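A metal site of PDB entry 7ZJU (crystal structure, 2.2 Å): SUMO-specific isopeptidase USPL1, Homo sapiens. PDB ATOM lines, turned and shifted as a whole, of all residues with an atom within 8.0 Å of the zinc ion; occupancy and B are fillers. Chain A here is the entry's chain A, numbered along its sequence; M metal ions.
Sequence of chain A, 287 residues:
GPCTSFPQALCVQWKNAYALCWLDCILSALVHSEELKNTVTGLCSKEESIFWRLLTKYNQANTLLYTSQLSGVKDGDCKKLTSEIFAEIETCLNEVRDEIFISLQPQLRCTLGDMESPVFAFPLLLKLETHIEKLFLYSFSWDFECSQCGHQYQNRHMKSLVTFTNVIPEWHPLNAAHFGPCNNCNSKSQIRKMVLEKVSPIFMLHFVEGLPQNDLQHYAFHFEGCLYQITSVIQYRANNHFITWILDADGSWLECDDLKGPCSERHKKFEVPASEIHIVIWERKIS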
ATOM      1  N   PHE A 144      -6.425   8.012  21.763  1.00  0.00           N
ATOM      2  CA  PHE A 144      -5.288   8.906  21.988  1.00  0.00           C
ATOM      3  C   PHE A 144      -5.733  10.345  21.795  1.00  0.00           C
ATOM      4  O   PHE A 144      -6.577  10.643  20.936  1.00  0.00           O
ATOM      5  CB  PHE A 144      -4.120   8.579  21.049  1.00  0.00           C
ATOM      6  CG  PHE A 144      -2.927   9.474  21.225  1.00  0.00           C
ATOM      7  CD1 PHE A 144      -1.925   9.151  22.125  1.00  0.00           C
ATOM      8  CD2 PHE A 144      -2.794  10.636  20.473  1.00  0.00           C
ATOM      9  CE1 PHE A 144      -0.819   9.983  22.287  1.00  0.00           C
ATOM     10  CE2 PHE A 144      -1.697  11.466  20.630  1.00  0.00           C
ATOM     11  CZ  PHE A 144      -0.710  11.139  21.537  1.00  0.00           C
ATOM     12  N   GLU A 145      -5.151  11.238  22.587  1.00  0.00           N
ATOM     13  CA  GLU A 145      -5.443  12.671  22.477  1.00  0.00           C
ATOM     14  C   GLU A 145      -4.270  13.435  23.061  1.00  0.00           C
ATOM     15  O   GLU A 145      -4.074  13.428  24.281  1.00  0.00           O
ATOM     16  CB  GLU A 145      -6.747  13.020  23.187  1.00  0.00           C
ATOM     17  CG  GLU A 145      -7.043  14.505  23.218  1.00  0.00           C
ATOM     18  CD  GLU A 145      -8.465  14.804  23.622  1.00  0.00           C
ATOM     19  OE1 GLU A 145      -9.195  15.451  22.835  1.00  0.00           O
ATOM     20  OE2 GLU A 145      -8.866  14.387  24.735  1.00  0.00           O
ATOM     21  N   CYS A 146      -3.496  14.084  22.197  1.00  0.00           N
ATOM     22  CA  CYS A 146      -2.335  14.836  22.654  1.00  0.00           C
ATOM     23  C   CYS A 146      -2.779  16.131  23.331  1.00  0.00           C
ATOM     24  O   CYS A 146      -3.696  16.817  22.863  1.00  0.00           O
ATOM     25  CB  CYS A 146      -1.407  15.148  21.482  1.00  0.00           C
ATOM     26  SG  CYS A 146       0.072  16.087  21.930  1.00  0.00           S
ATOM     27  N   SER A 147      -2.135  16.459  24.445  1.00  0.00           N
ATOM     28  CA  SER A 147      -2.387  17.723  25.132  1.00  0.00           C
ATOM     29  C   SER A 147      -1.526  18.855  24.606  1.00  0.00           C
ATOM     30  O   SER A 147      -1.880  20.023  24.805  1.00  0.00           O
ATOM     31  CB  SER A 147      -2.174  17.563  26.637  1.00  0.00           C
ATOM     32  OG  SER A 147      -0.802  17.693  26.971  1.00  0.00           O
ATOM     33  N   GLN A 148      -0.408  18.542  23.949  1.00  0.00           N
ATOM     34  CA  GLN A 148       0.469  19.584  23.425  1.00  0.00           C
ATOM     35  C   GLN A 148      -0.082  20.162  22.115  1.00  0.00           C
ATOM     36  O   GLN A 148      -0.236  21.380  21.985  1.00  0.00           O
ATOM     37  CB  GLN A 148       1.876  19.027  23.217  1.00  0.00           C
ATOM     38  N   CYS A 149      -0.361  19.307  21.137  1.00  0.00           N
ATOM     39  CA  CYS A 149      -1.040  19.693  19.917  1.00  0.00           C
ATOM     40  C   CYS A 149      -2.443  19.078  19.930  1.00  0.00           C
ATOM     41  O   CYS A 149      -2.868  18.472  20.912  1.00  0.00           O
ATOM     42  CB  CYS A 149      -0.225  19.278  18.691  1.00  0.00           C
ATOM     43  SG  CYS A 149      -0.096  17.507  18.409  1.00  0.00           S
ATOM     44  N   GLY A 150      -3.159  19.226  18.822  1.00  0.00           N
ATOM     45  CA  GLY A 150      -4.509  18.706  18.759  1.00  0.00           C
ATOM     46  C   GLY A 150      -4.642  17.274  18.311  1.00  0.00           C
ATOM     47  O   GLY A 150      -5.773  16.767  18.223  1.00  0.00           O
ATOM     48  N   HIS A 151      -3.522  16.590  18.066  1.00  0.00           N
ATOM     49  CA  HIS A 151      -3.558  15.274  17.430  1.00  0.00           C
ATOM     50  C   HIS A 151      -4.356  14.274  18.252  1.00  0.00           C
ATOM     51  O   HIS A 151      -4.103  14.099  19.452  1.00  0.00           O
ATOM     52  CB  HIS A 151      -2.125  14.773  17.223  1.00  0.00           C
ATOM     53  CG  HIS A 151      -2.051  13.432  16.574  1.00  0.00           C
ATOM     54  ND1 HIS A 151      -2.469  13.197  15.286  1.00  0.00           N
ATOM     55  CD2 HIS A 151      -1.583  12.241  17.033  1.00  0.00           C
ATOM     56  CE1 HIS A 151      -2.274  11.927  14.972  1.00  0.00           C
ATOM     57  NE2 HIS A 151      -1.734  11.329  16.022  1.00  0.00           N
ATOM     58  N   GLN A 152      -5.320  13.624  17.605  1.00  0.00           N
ATOM     59  CA  GLN A 152      -6.148  12.617  18.249  1.00  0.00           C
ATOM     60  C   GLN A 152      -6.550  11.570  17.221  1.00  0.00           C
ATOM     61  O   GLN A 152      -6.662  11.863  16.027  1.00  0.00           O
ATOM     62  CB  GLN A 152      -7.394  13.236  18.882  1.00  0.00           C
ATOM     63  N   PRO A 181       4.461   8.686  23.489  1.00  0.00           N
ATOM     64  CA  PRO A 181       4.738   9.923  22.754  1.00  0.00           C
ATOM     65  C   PRO A 181       3.666  10.222  21.724  1.00  0.00           C
ATOM     66  O   PRO A 181       2.864   9.364  21.339  1.00  0.00           O
ATOM     67  CB  PRO A 181       6.087   9.640  22.083  1.00  0.00           C
ATOM     68  CG  PRO A 181       6.092   8.163  21.903  1.00  0.00           C
ATOM     69  CD  PRO A 181       5.320   7.576  23.046  1.00  0.00           C
ATOM     70  N   CYS A 182       3.655  11.470  21.267  1.00  0.00           N
ATOM     71  CA  CYS A 182       2.752  11.908  20.213  1.00  0.00           C
ATOM     72  C   CYS A 182       3.484  11.893  18.882  1.00  0.00           C
ATOM     73  O   CYS A 182       4.569  12.464  18.760  1.00  0.00           O
ATOM     74  CB  CYS A 182       2.211  13.313  20.499  1.00  0.00           C
ATOM     75  SG  CYS A 182       1.412  14.073  19.071  1.00  0.00           S
ATOM     76  N   ASN A 183       2.890  11.245  17.883  1.00  0.00           N
ATOM     77  CA  ASN A 183       3.509  11.124  16.573  1.00  0.00           C
ATOM     78  C   ASN A 183       3.521  12.427  15.798  1.00  0.00           C
ATOM     79  O   ASN A 183       4.227  12.517  14.778  1.00  0.00           O
ATOM     80  CB  ASN A 183       2.783  10.041  15.761  1.00  0.00           C
ATOM     81  CG  ASN A 183       2.923   8.669  16.375  1.00  0.00           C
ATOM     82  OD1 ASN A 183       3.992   8.278  16.835  1.00  0.00           O
ATOM     83  ND2 ASN A 183       1.818   7.917  16.394  1.00  0.00           N
ATOM     84  N   ASN A 184       2.771  13.439  16.231  1.00  0.00           N
ATOM     85  CA  ASN A 184       2.649  14.703  15.510  1.00  0.00           C
ATOM     86  C   ASN A 184       3.626  15.762  15.993  1.00  0.00           C
ATOM     87  O   ASN A 184       4.144  16.533  15.171  1.00  0.00           O
ATOM     88  CB  ASN A 184       1.219  15.230  15.631  1.00  0.00           C
ATOM     89  CG  ASN A 184       0.807  16.079  14.453  1.00  0.00           C
ATOM     90  OD1 ASN A 184       1.232  15.843  13.315  1.00  0.00           O
ATOM     91  ND2 ASN A 184      -0.018  17.082  14.706  1.00  0.00           N
ATOM     92  N   CYS A 185       3.889  15.831  17.292  1.00  0.00           N
ATOM     93  CA  CYS A 185       4.739  16.873  17.846  1.00  0.00           C
ATOM     94  C   CYS A 185       5.872  16.334  18.721  1.00  0.00           C
ATOM     95  O   CYS A 185       6.613  17.141  19.292  1.00  0.00           O
ATOM     96  CB  CYS A 185       3.906  17.866  18.660  1.00  0.00           C
ATOM     97  SG  CYS A 185       3.265  17.204  20.204  1.00  0.00           S
ATOM     98  N   ASN A 186       6.015  15.013  18.843  1.00  0.00           N
ATOM     99  CA  ASN A 186       7.093  14.372  19.592  1.00  0.00           C
ATOM    100  C   ASN A 186       7.073  14.726  21.078  1.00  0.00           C
ATOM    101  O   ASN A 186       8.082  14.566  21.769  1.00  0.00           O
ATOM    102  CB  ASN A 186       8.461  14.699  18.988  1.00  0.00           C
ATOM    103  CG  ASN A 186       8.748  13.886  17.750  1.00  0.00           C
ATOM    104  OD1 ASN A 186       8.768  14.415  16.635  1.00  0.00           O
ATOM    105  ND2 ASN A 186       8.985  12.590  17.925  1.00  0.00           N
ATOM    106  N   SER A 187       5.944  15.202  21.590  1.00  0.00           N
ATOM    107  CA  SER A 187       5.805  15.380  23.033  1.00  0.00           C
ATOM    108  C   SER A 187       5.710  14.027  23.708  1.00  0.00           C
ATOM    109  O   SER A 187       5.032  13.114  23.222  1.00  0.00           O
ATOM    110  CB  SER A 187       4.571  16.225  23.354  1.00  0.00           C
ATOM    111  N   LYS A 188       6.400  13.886  24.836  1.00  0.00           N
ATOM    112  CA  LYS A 188       6.405  12.646  25.583  1.00  0.00           C
ATOM    113  C   LYS A 188       5.406  12.704  26.735  1.00  0.00           C
ATOM    114  O   LYS A 188       4.873  13.768  27.075  1.00  0.00           O
ATOM    115  CB  LYS A 188       7.819  12.342  26.117  1.00  0.00           C
ATOM    116  N   GLN A 190       2.398  11.720  26.925  1.00  0.00           N
ATOM    117  CA  GLN A 190       0.969  11.706  26.644  1.00  0.00           C
ATOM    118  C   GLN A 190       0.412  10.329  26.994  1.00  0.00           C
ATOM    119  O   GLN A 190       1.164   9.396  27.269  1.00  0.00           O
ATOM    120  CB  GLN A 190       0.697  12.068  25.189  1.00  0.00           C
ATOM    121  CG  GLN A 190       1.317  13.383  24.741  1.00  0.00           C
ATOM    122  CD  GLN A 190       0.642  14.592  25.372  1.00  0.00           C
ATOM    123  OE1 GLN A 190      -0.563  14.585  25.586  1.00  0.00           O
ATOM    124  NE2 GLN A 190       1.418  15.621  25.670  1.00  0.00           N
HETATM  125 ZN    ZN M   1       1.163  16.259  19.905  1.00  0.00          ZN
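SG of Cys 146 sits close to N of Gln 148 (3.2 Å). N of Cys 146 sits at hydrogen-bond distance from O of His 151, 2.8 Å away. The side-chain sulfur (SG) of Cys 149 sits close to the side-chain amide nitrogen (ND2) of Asn 184 (3.7 Å). The side-chain sulfur of Cys 149 lies close to the backbone NH of His 151. The side-chain sulfur (SG) of Cys 185 lies close to the backbone NH (N) of Ser 187 (3.6 Å). The side-chain sulfur (SG) of Cys 182 lies close to the backbone NH (N) of Asn 184, at 3.2 Å. The backbone carbonyl oxygen of Ser 187 lies within hydrogen-bond range of the backbone NH of Cys 182, 2.9 Å away.
Within 4 Å of the zinc ion: Cys 146, Cys 149, Cys 182 and Cys 185.
The zinc ion is bound by the side-chain sulfur (SG) of Cys 146. SG of Cys 149 binds the zinc ion, 2.3 Å away. SG of Cys 185 is bound to the zinc ion (2.3 Å). SG of Cys 182 binds the zinc ion (2.4 Å).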
